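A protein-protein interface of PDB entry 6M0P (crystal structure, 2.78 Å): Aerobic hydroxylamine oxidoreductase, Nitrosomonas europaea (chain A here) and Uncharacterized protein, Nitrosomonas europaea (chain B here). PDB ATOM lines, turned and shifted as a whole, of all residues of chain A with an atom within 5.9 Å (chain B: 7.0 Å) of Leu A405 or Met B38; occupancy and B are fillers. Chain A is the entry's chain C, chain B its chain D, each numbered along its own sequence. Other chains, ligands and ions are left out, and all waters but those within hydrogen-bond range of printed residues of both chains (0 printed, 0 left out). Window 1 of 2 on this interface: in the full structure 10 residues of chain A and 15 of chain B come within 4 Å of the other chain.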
ATOM      1  N   TRP A 355       8.409   6.885  -2.797  1.00  0.00           N
ATOM      2  CA  TRP A 355       9.189   6.444  -1.646  1.00  0.00           C
ATOM      3  C   TRP A 355      10.629   6.095  -1.991  1.00  0.00           C
ATOM      4  O   TRP A 355      11.515   6.264  -1.144  1.00  0.00           O
ATOM      5  CB  TRP A 355       8.529   5.226  -0.995  1.00  0.00           C
ATOM      6  CG  TRP A 355       7.370   5.554  -0.113  1.00  0.00           C
ATOM      7  CD1 TRP A 355       6.048   5.479  -0.432  1.00  0.00           C
ATOM      8  CD2 TRP A 355       7.432   6.001   1.247  1.00  0.00           C
ATOM      9  NE1 TRP A 355       5.280   5.856   0.643  1.00  0.00           N
ATOM     10  CE2 TRP A 355       6.107   6.183   1.686  1.00  0.00           C
ATOM     11  CE3 TRP A 355       8.479   6.269   2.132  1.00  0.00           C
ATOM     12  CZ2 TRP A 355       5.801   6.618   2.973  1.00  0.00           C
ATOM     13  CZ3 TRP A 355       8.173   6.701   3.408  1.00  0.00           C
ATOM     14  CH2 TRP A 355       6.846   6.871   3.817  1.00  0.00           C
ATOM     15  N   ALA A 365       9.876  10.850   3.741  1.00  0.00           N
ATOM     16  CA  ALA A 365       8.642  10.711   4.506  1.00  0.00           C
ATOM     17  C   ALA A 365       7.879  12.027   4.577  1.00  0.00           C
ATOM     18  O   ALA A 365       6.653  12.052   4.420  1.00  0.00           O
ATOM     19  CB  ALA A 365       8.952  10.200   5.912  1.00  0.00           C
ATOM     20  N   GLU A 366       8.589  13.132   4.810  1.00  0.00           N
ATOM     21  CA  GLU A 366       7.943  14.434   4.917  1.00  0.00           C
ATOM     22  C   GLU A 366       7.325  14.887   3.600  1.00  0.00           C
ATOM     23  O   GLU A 366       6.430  15.739   3.611  1.00  0.00           O
ATOM     24  CB  GLU A 366       8.951  15.473   5.409  1.00  0.00           C
ATOM     25  CG  GLU A 366       9.611  15.131   6.745  1.00  0.00           C
ATOM     26  CD  GLU A 366      10.821  14.220   6.601  1.00  0.00           C
ATOM     27  OE1 GLU A 366      10.909  13.490   5.591  1.00  0.00           O
ATOM     28  OE2 GLU A 366      11.686  14.234   7.502  1.00  0.00           O
ATOM     29  N   ASN A 367       7.775  14.337   2.473  1.00  0.00           N
ATOM     30  CA  ASN A 367       7.262  14.704   1.161  1.00  0.00           C
ATOM     31  C   ASN A 367       6.072  13.855   0.727  1.00  0.00           C
ATOM     32  O   ASN A 367       5.452  14.162  -0.297  1.00  0.00           O
ATOM     33  CB  ASN A 367       8.385  14.597   0.118  1.00  0.00           C
ATOM     34  CG  ASN A 367       8.001  15.185  -1.224  1.00  0.00           C
ATOM     35  OD1 ASN A 367       7.749  14.456  -2.182  1.00  0.00           O
ATOM     36  ND2 ASN A 367       7.955  16.510  -1.298  1.00  0.00           N
ATOM     37  N   ILE A 368       5.728  12.811   1.484  1.00  0.00           N
ATOM     38  CA  ILE A 368       4.679  11.895   1.055  1.00  0.00           C
ATOM     39  C   ILE A 368       3.301  12.549   1.052  1.00  0.00           C
ATOM     40  O   ILE A 368       2.385  12.045   0.394  1.00  0.00           O
ATOM     41  CB  ILE A 368       4.686  10.629   1.932  1.00  0.00           C
ATOM     42  CG1 ILE A 368       4.148   9.439   1.139  1.00  0.00           C
ATOM     43  CG2 ILE A 368       3.867  10.842   3.196  1.00  0.00           C
ATOM     44  CD1 ILE A 368       4.967   9.113  -0.088  1.00  0.00           C
ATOM     45  N   THR A 369       3.124  13.662   1.765  1.00  0.00           N
ATOM     46  CA  THR A 369       1.852  14.373   1.780  1.00  0.00           C
ATOM     47  C   THR A 369       1.840  15.582   0.855  1.00  0.00           C
ATOM     48  O   THR A 369       0.829  16.287   0.793  1.00  0.00           O
ATOM     49  CB  THR A 369       1.500  14.817   3.206  1.00  0.00           C
ATOM     50  OG1 THR A 369       2.471  15.760   3.676  1.00  0.00           O
ATOM     51  CG2 THR A 369       1.469  13.623   4.142  1.00  0.00           C
ATOM     52  N   MET A 400      -0.062   1.263   2.600  1.00  0.00           N
ATOM     53  CA  MET A 400       1.349   1.244   2.236  1.00  0.00           C
ATOM     54  C   MET A 400       2.084   2.454   2.799  1.00  0.00           C
ATOM     55  O   MET A 400       3.196   2.325   3.324  1.00  0.00           O
ATOM     56  CB  MET A 400       1.489   1.193   0.716  1.00  0.00           C
ATOM     57  CG  MET A 400       2.912   1.312   0.211  1.00  0.00           C
ATOM     58  SD  MET A 400       2.951   1.608  -1.565  1.00  0.00           S
ATOM     59  CE  MET A 400       2.093   3.175  -1.672  1.00  0.00           C
ATOM     60  N   ASP A 401       1.478   3.640   2.702  1.00  0.00           N
ATOM     61  CA  ASP A 401       2.130   4.845   3.204  1.00  0.00           C
ATOM     62  C   ASP A 401       2.230   4.823   4.724  1.00  0.00           C
ATOM     63  O   ASP A 401       3.306   5.049   5.290  1.00  0.00           O
ATOM     64  CB  ASP A 401       1.373   6.087   2.736  1.00  0.00           C
ATOM     65  CG  ASP A 401       1.512   6.328   1.248  1.00  0.00           C
ATOM     66  OD1 ASP A 401       2.262   5.578   0.588  1.00  0.00           O
ATOM     67  OD2 ASP A 401       0.874   7.273   0.736  1.00  0.00           O
ATOM     68  N   LYS A 402       1.112   4.555   5.402  1.00  0.00           N
ATOM     69  CA  LYS A 402       1.118   4.526   6.860  1.00  0.00           C
ATOM     70  C   LYS A 402       1.914   3.339   7.389  1.00  0.00           C
ATOM     71  O   LYS A 402       2.593   3.449   8.416  1.00  0.00           O
ATOM     72  CB  LYS A 402      -0.318   4.504   7.386  1.00  0.00           C
ATOM     73  CG  LYS A 402      -1.091   5.772   7.058  1.00  0.00           C
ATOM     74  CD  LYS A 402      -2.505   5.745   7.609  1.00  0.00           C
ATOM     75  CE  LYS A 402      -3.241   7.025   7.244  1.00  0.00           C
ATOM     76  NZ  LYS A 402      -4.648   7.029   7.727  1.00  0.00           N
ATOM     77  N   GLY A 403       1.842   2.196   6.706  1.00  0.00           N
ATOM     78  CA  GLY A 403       2.627   1.048   7.129  1.00  0.00           C
ATOM     79  C   GLY A 403       4.119   1.286   7.000  1.00  0.00           C
ATOM     80  O   GLY A 403       4.909   0.809   7.820  1.00  0.00           O
ATOM     81  N   THR A 404       4.528   2.017   5.963  1.00  0.00           N
ATOM     82  CA  THR A 404       5.936   2.359   5.808  1.00  0.00           C
ATOM     83  C   THR A 404       6.389   3.328   6.892  1.00  0.00           C
ATOM     84  O   THR A 404       7.501   3.205   7.420  1.00  0.00           O
ATOM     85  CB  THR A 404       6.177   2.947   4.418  1.00  0.00           C
ATOM     86  OG1 THR A 404       5.689   2.036   3.425  1.00  0.00           O
ATOM     87  CG2 THR A 404       7.652   3.186   4.189  1.00  0.00           C
ATOM     88  N   LEU A 405       5.537   4.292   7.245  1.00  0.00           N
ATOM     89  CA  LEU A 405       5.879   5.225   8.313  1.00  0.00           C
ATOM     90  C   LEU A 405       5.936   4.536   9.669  1.00  0.00           C
ATOM     91  O   LEU A 405       6.750   4.917  10.520  1.00  0.00           O
ATOM     92  CB  LEU A 405       4.873   6.375   8.351  1.00  0.00           C
ATOM     93  CG  LEU A 405       4.857   7.334   7.163  1.00  0.00           C
ATOM     94  CD1 LEU A 405       3.694   8.304   7.287  1.00  0.00           C
ATOM     95  CD2 LEU A 405       6.175   8.082   7.080  1.00  0.00           C
ATOM     96  N   GLU A 406       5.086   3.532   9.894  1.00  0.00           N
ATOM     97  CA  GLU A 406       5.132   2.804  11.158  1.00  0.00           C
ATOM     98  C   GLU A 406       6.457   2.074  11.315  1.00  0.00           C
ATOM     99  O   GLU A 406       7.029   2.035  12.411  1.00  0.00           O
ATOM    100  CB  GLU A 406       3.959   1.828  11.245  1.00  0.00           C
ATOM    101  CG  GLU A 406       2.627   2.510  11.513  1.00  0.00           C
ATOM    102  CD  GLU A 406       1.431   1.640  11.177  1.00  0.00           C
ATOM    103  OE1 GLU A 406       1.620   0.461  10.816  1.00  0.00           O
ATOM    104  OE2 GLU A 406       0.295   2.146  11.279  1.00  0.00           O
ATOM    105  N   GLY A 407       6.967   1.498  10.226  1.00  0.00           N
ATOM    106  CA  GLY A 407       8.293   0.910  10.272  1.00  0.00           C
ATOM    107  C   GLY A 407       9.381   1.958  10.408  1.00  0.00           C
ATOM    108  O   GLY A 407      10.351   1.766  11.144  1.00  0.00           O
ATOM    109  N   LEU A 408       9.233   3.081   9.700  1.00  0.00           N
ATOM    110  CA  LEU A 408      10.231   4.142   9.786  1.00  0.00           C
ATOM    111  C   LEU A 408      10.372   4.656  11.213  1.00  0.00           C
ATOM    112  O   LEU A 408      11.491   4.872  11.695  1.00  0.00           O
ATOM    113  CB  LEU A 408       9.861   5.285   8.841  1.00  0.00           C
ATOM    114  CG  LEU A 408      10.783   6.504   8.891  1.00  0.00           C
ATOM    115  CD1 LEU A 408      12.201   6.114   8.511  1.00  0.00           C
ATOM    116  CD2 LEU A 408      10.266   7.604   7.987  1.00  0.00           C
ATOM    117  N   ALA A 409       9.250   4.852  11.908  1.00  0.00           N
ATOM    118  CA  ALA A 409       9.310   5.320  13.288  1.00  0.00           C
ATOM    119  C   ALA A 409       9.974   4.298  14.200  1.00  0.00           C
ATOM    120  O   ALA A 409      10.640   4.674  15.171  1.00  0.00           O
ATOM    121  CB  ALA A 409       7.905   5.652  13.794  1.00  0.00           C
ATOM    122  N   LYS A 410       9.811   3.007  13.901  1.00  0.00           N
ATOM    123  CA  LYS A 410      10.454   1.972  14.704  1.00  0.00           C
ATOM    124  C   LYS A 410      11.972   2.066  14.606  1.00  0.00           C
ATOM    125  O   LYS A 410      12.677   1.909  15.609  1.00  0.00           O
ATOM    126  CB  LYS A 410       9.965   0.592  14.260  1.00  0.00           C
ATOM    127  CG  LYS A 410      10.382  -0.553  15.169  1.00  0.00           C
ATOM    128  CD  LYS A 410       9.709  -0.464  16.523  1.00  0.00           C
ATOM    129  CE  LYS A 410      10.048  -1.672  17.378  1.00  0.00           C
ATOM    130  NZ  LYS A 410       9.341  -1.650  18.689  1.00  0.00           N
ATOM    131  N   ILE B  33      10.697  15.916   9.979  1.00  0.00           N
ATOM    132  CA  ILE B  33       9.538  15.559  10.791  1.00  0.00           C
ATOM    133  C   ILE B  33       9.614  14.065  11.068  1.00  0.00           C
ATOM    134  O   ILE B  33       9.763  13.264  10.139  1.00  0.00           O
ATOM    135  CB  ILE B  33       8.207  15.910  10.097  1.00  0.00           C
ATOM    136  CG1 ILE B  33       8.106  17.418   9.853  1.00  0.00           C
ATOM    137  CG2 ILE B  33       7.026  15.415  10.922  1.00  0.00           C
ATOM    138  CD1 ILE B  33       6.857  17.834   9.105  1.00  0.00           C
ATOM    139  N   SER B  34       9.516  13.690  12.340  1.00  0.00           N
ATOM    140  CA  SER B  34       9.598  12.285  12.711  1.00  0.00           C
ATOM    141  C   SER B  34       8.408  11.507  12.163  1.00  0.00           C
ATOM    142  O   SER B  34       7.332  12.059  11.915  1.00  0.00           O
ATOM    143  CB  SER B  34       9.667  12.136  14.230  1.00  0.00           C
ATOM    144  OG  SER B  34       8.492  12.634  14.844  1.00  0.00           O
ATOM    145  N   ALA B  35       8.615  10.202  11.972  1.00  0.00           N
ATOM    146  CA  ALA B  35       7.571   9.368  11.387  1.00  0.00           C
ATOM    147  C   ALA B  35       6.367   9.245  12.309  1.00  0.00           C
ATOM    148  O   ALA B  35       5.234   9.112  11.831  1.00  0.00           O
ATOM    149  CB  ALA B  35       8.127   7.986  11.047  1.00  0.00           C
ATOM    150  N   LYS B  36       6.584   9.280  13.627  1.00  0.00           N
ATOM    151  CA  LYS B  36       5.456   9.266  14.551  1.00  0.00           C
ATOM    152  C   LYS B  36       4.596  10.512  14.392  1.00  0.00           C
ATOM    153  O   LYS B  36       3.371  10.446  14.552  1.00  0.00           O
ATOM    154  CB  LYS B  36       5.950   9.146  15.992  1.00  0.00           C
ATOM    155  CG  LYS B  36       6.942  10.221  16.401  1.00  0.00           C
ATOM    156  CD  LYS B  36       7.164  10.231  17.903  1.00  0.00           C
ATOM    157  CE  LYS B  36       5.933  10.749  18.630  1.00  0.00           C
ATOM    158  NZ  LYS B  36       5.628  12.158  18.255  1.00  0.00           N
ATOM    159  N   ASP B  37       5.213  11.650  14.069  1.00  0.00           N
ATOM    160  CA  ASP B  37       4.447  12.870  13.840  1.00  0.00           C
ATOM    161  C   ASP B  37       3.734  12.838  12.496  1.00  0.00           C
ATOM    162  O   ASP B  37       2.608  13.332  12.376  1.00  0.00           O
ATOM    163  CB  ASP B  37       5.366  14.090  13.929  1.00  0.00           C
ATOM    164  CG  ASP B  37       5.953  14.281  15.314  1.00  0.00           C
ATOM    165  OD1 ASP B  37       5.268  13.943  16.302  1.00  0.00           O
ATOM    166  OD2 ASP B  37       7.095  14.771  15.418  1.00  0.00           O
ATOM    167  N   MET B  38       4.364  12.248  11.477  1.00  0.00           N
ATOM    168  CA  MET B  38       3.700  12.103  10.186  1.00  0.00           C
ATOM    169  C   MET B  38       2.455  11.234  10.300  1.00  0.00           C
ATOM    170  O   MET B  38       1.427  11.523   9.675  1.00  0.00           O
ATOM    171  CB  MET B  38       4.669  11.525   9.157  1.00  0.00           C
ATOM    172  CG  MET B  38       5.789  12.475   8.781  1.00  0.00           C
ATOM    173  SD  MET B  38       5.169  13.928   7.916  1.00  0.00           S
ATOM    174  CE  MET B  38       4.342  13.169   6.521  1.00  0.00           C
ATOM    175  N   LEU B  39       2.524  10.167  11.100  1.00  0.00           N
ATOM    176  CA  LEU B  39       1.371   9.287  11.250  1.00  0.00           C
ATOM    177  C   LEU B  39       0.246   9.977  12.007  1.00  0.00           C
ATOM    178  O   LEU B  39      -0.926   9.849  11.638  1.00  0.00           O
ATOM    179  CB  LEU B  39       1.785   7.996  11.952  1.00  0.00           C
ATOM    180  CG  LEU B  39       2.624   7.048  11.098  1.00  0.00           C
ATOM    181  CD1 LEU B  39       3.336   6.031  11.965  1.00  0.00           C
ATOM    182  CD2 LEU B  39       1.739   6.353  10.078  1.00  0.00           C
ATOM    183  N   ASP B  40       0.580  10.712  13.070  1.00  0.00           N
ATOM    184  CA  ASP B  40      -0.445  11.468  13.778  1.00  0.00           C
ATOM    185  C   ASP B  40      -1.014  12.576  12.903  1.00  0.00           C
ATOM    186  O   ASP B  40      -2.190  12.934  13.039  1.00  0.00           O
ATOM    187  CB  ASP B  40       0.128  12.050  15.070  1.00  0.00           C
ATOM    188  CG  ASP B  40       0.713  10.986  15.980  1.00  0.00           C
ATOM    189  OD1 ASP B  40       0.360   9.799  15.816  1.00  0.00           O
ATOM    190  OD2 ASP B  40       1.526  11.339  16.860  1.00  0.00           O
ATOM    191  N   TYR B  41      -0.204  13.120  11.994  1.00  0.00           N
ATOM    192  CA  TYR B  41      -0.709  14.110  11.049  1.00  0.00           C
ATOM    193  C   TYR B  41      -1.612  13.458  10.012  1.00  0.00           C
ATOM    194  O   TYR B  41      -2.656  14.012   9.648  1.00  0.00           O
ATOM    195  CB  TYR B  41       0.458  14.834  10.380  1.00  0.00           C
ATOM    196  CG  TYR B  41       0.058  15.817   9.305  1.00  0.00           C
ATOM    197  CD1 TYR B  41      -0.413  17.082   9.633  1.00  0.00           C
ATOM    198  CD2 TYR B  41       0.163  15.485   7.960  1.00  0.00           C
ATOM    199  CE1 TYR B  41      -0.776  17.988   8.651  1.00  0.00           C
ATOM    200  CE2 TYR B  41      -0.196  16.384   6.971  1.00  0.00           C
ATOM    201  CZ  TYR B  41      -0.665  17.633   7.323  1.00  0.00           C
ATOM    202  OH  TYR B  41      -1.023  18.527   6.340  1.00  0.00           O
ATOM    203  N   LEU B  42      -1.221  12.282   9.519  1.00  0.00           N
ATOM    204  CA  LEU B  42      -2.043  11.565   8.551  1.00  0.00           C
ATOM    205  C   LEU B  42      -3.336  11.057   9.174  1.00  0.00           C
ATOM    206  O   LEU B  42      -4.366  10.990   8.493  1.00  0.00           O
ATOM    207  CB  LEU B  42      -1.252  10.401   7.959  1.00  0.00           C
ATOM    208  CG  LEU B  42      -0.436  10.700   6.703  1.00  0.00           C
ATOM    209  CD1 LEU B  42       0.268   9.440   6.230  1.00  0.00           C
ATOM    210  CD2 LEU B  42      -1.319  11.273   5.609  1.00  0.00           C
ATOM    211  N   ALA B  43      -3.304  10.685  10.456  1.00  0.00           N
ATOM    212  CA  ALA B  43      -4.502  10.198  11.129  1.00  0.00           C
ATOM    213  C   ALA B  43      -5.484  11.313  11.455  1.00  0.00           C
ATOM    214  O   ALA B  43      -6.651  11.030  11.739  1.00  0.00           O
ATOM    215  CB  ALA B  43      -4.121   9.454  12.409  1.00  0.00           C
ATOM    216  N   CYS B  44      -5.043  12.567  11.414  1.00  0.00           N
ATOM    217  CA  CYS B  44      -5.887  13.708  11.739  1.00  0.00           C
ATOM    218  C   CYS B  44      -6.417  14.427  10.510  1.00  0.00           C
ATOM    219  O   CYS B  44      -7.111  15.440  10.654  1.00  0.00           O
ATOM    220  CB  CYS B  44      -5.122  14.690  12.628  1.00  0.00           C
ATOM    221  SG  CYS B  44      -4.977  14.141  14.340  1.00  0.00           S
ATOM    222  N   THR B  57       2.291   4.556  16.611  1.00  0.00           N
ATOM    223  CA  THR B  57       3.564   3.970  17.021  1.00  0.00           C
ATOM    224  C   THR B  57       3.855   4.071  18.512  1.00  0.00           C
ATOM    225  O   THR B  57       4.610   3.236  19.021  1.00  0.00           O
ATOM    226  CB  THR B  57       4.727   4.618  16.257  1.00  0.00           C
ATOM    227  OG1 THR B  57       4.648   6.044  16.383  1.00  0.00           O
ATOM    228  CG2 THR B  57       4.695   4.228  14.787  1.00  0.00           C
ATOM    229  N   ILE B  72      -0.836  18.212  16.729  1.00  0.00           N
ATOM    230  CA  ILE B  72       0.030  17.612  15.720  1.00  0.00           C
ATOM    231  C   ILE B  72       0.037  18.458  14.450  1.00  0.00           C
ATOM    232  O   ILE B  72       1.082  18.632  13.812  1.00  0.00           O
ATOM    233  CB  ILE B  72      -0.392  16.156  15.442  1.00  0.00           C
ATOM    234  CG1 ILE B  72       0.455  15.563  14.315  1.00  0.00           C
ATOM    235  CG2 ILE B  72      -1.873  16.067  15.116  1.00  0.00           C
ATOM    236  CD1 ILE B  72       1.939  15.532  14.620  1.00  0.00           C
ATOM    237  N   VAL B  76       3.278  20.240  12.785  1.00  0.00           N
ATOM    238  CA  VAL B  76       3.712  20.076  11.402  1.00  0.00           C
ATOM    239  C   VAL B  76       3.844  21.429  10.716  1.00  0.00           C
ATOM    240  O   VAL B  76       4.825  21.685  10.009  1.00  0.00           O
ATOM    241  CB  VAL B  76       2.742  19.147  10.650  1.00  0.00           C
ATOM    242  CG1 VAL B  76       3.063  19.133   9.163  1.00  0.00           C
ATOM    243  CG2 VAL B  76       2.807  17.741  11.222  1.00  0.00           C
ATOM    244  N   ARG B  80       6.893  23.379   8.696  1.00  0.00           N
ATOM    245  CA  ARG B  80       6.794  23.758   7.291  1.00  0.00           C
ATOM    246  C   ARG B  80       7.161  25.220   7.079  1.00  0.00           C
ATOM    247  O   ARG B  80       7.705  25.572   6.026  1.00  0.00           O
ATOM    248  CB  ARG B  80       5.388  23.470   6.762  1.00  0.00           C
ATOM    249  CG  ARG B  80       5.011  21.997   6.797  1.00  0.00           C
ATOM    250  CD  ARG B  80       5.865  21.183   5.832  1.00  0.00           C
ATOM    251  NE  ARG B  80       5.534  19.761   5.870  1.00  0.00           N
ATOM    252  CZ  ARG B  80       4.598  19.187   5.120  1.00  0.00           C
ATOM    253  NH1 ARG B  80       3.891  19.914   4.264  1.00  0.00           N
ATOM    254  NH2 ARG B  80       4.367  17.886   5.227  1.00  0.00           N
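OE2 of Glu A366 is in hydrogen-bond range of N of Ile B33 (3.2 Å).
NH2 of Arg B80 is in hydrogen-bond range of O of Glu A366, at 3.4 Å.
The guanidinium group of Arg B80 is in hydrogen-bond range of the side-chain hydroxyl of Thr A369.
OD1 of Asp B37 is in salt-bridge range of NZ of Lys B36 (2.7 Å).
Among the printed residues, pairs that only touch across the chains: Ala A365 with Met B38, Leu A405 with Ala B35, Ala A409 with Ala B35, Lys A402 with Leu B39, Leu A405 with Leu B39, Glu A406 with Leu B39, Ala A409 with Thr B57, Leu A408 with Ala B35, Thr A369 with Met B38, Leu A405 with Leu B42, Leu A405 with Met B38, Ala A409 with Lys B36, Glu A406 with Thr B57, Thr A369 with Leu B42 and Lys A402 with Leu B42.
Printed residues of chain B within 4 Å of Ala A365: Met B38.
Of the printed residues of chain B, Thr A369 touches Met B38, Leu B42 and Arg B80.
Of the printed residues of chain B, Lys A402 touches Leu B39 and Leu B42.
Thr A404 touches none of the printed residues of chain B.
Of the printed residues of chain B, Leu A405 touches Ala B35, Met B38, Leu B39 and Leu B42.
Of chain A, only Ala A365, Thr A369 and Leu A405 come within 4 Å of Met B38.
Printed residues of chain A that touch a printed residue of chain B: Ala A365, Glu A366, Thr A369, Lys A402, Leu A405, Glu A406, Leu A408 and Ala A409.
Hydrophobic or aromatic side chains of chain B that line the printed part of chain A: Ile B33, Ala B35, Met B38, Leu B39 and Leu B42.
Along chain B the printed residues that touch a printed residue of chain A span positions 33 to 80.
Among the printed residues, 18 pairs touch across the chains.
Among the printed residues, no Asp or Glu carboxylate lies within 4 Å of a Lys or Arg side-chain nitrogen of the other chain.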
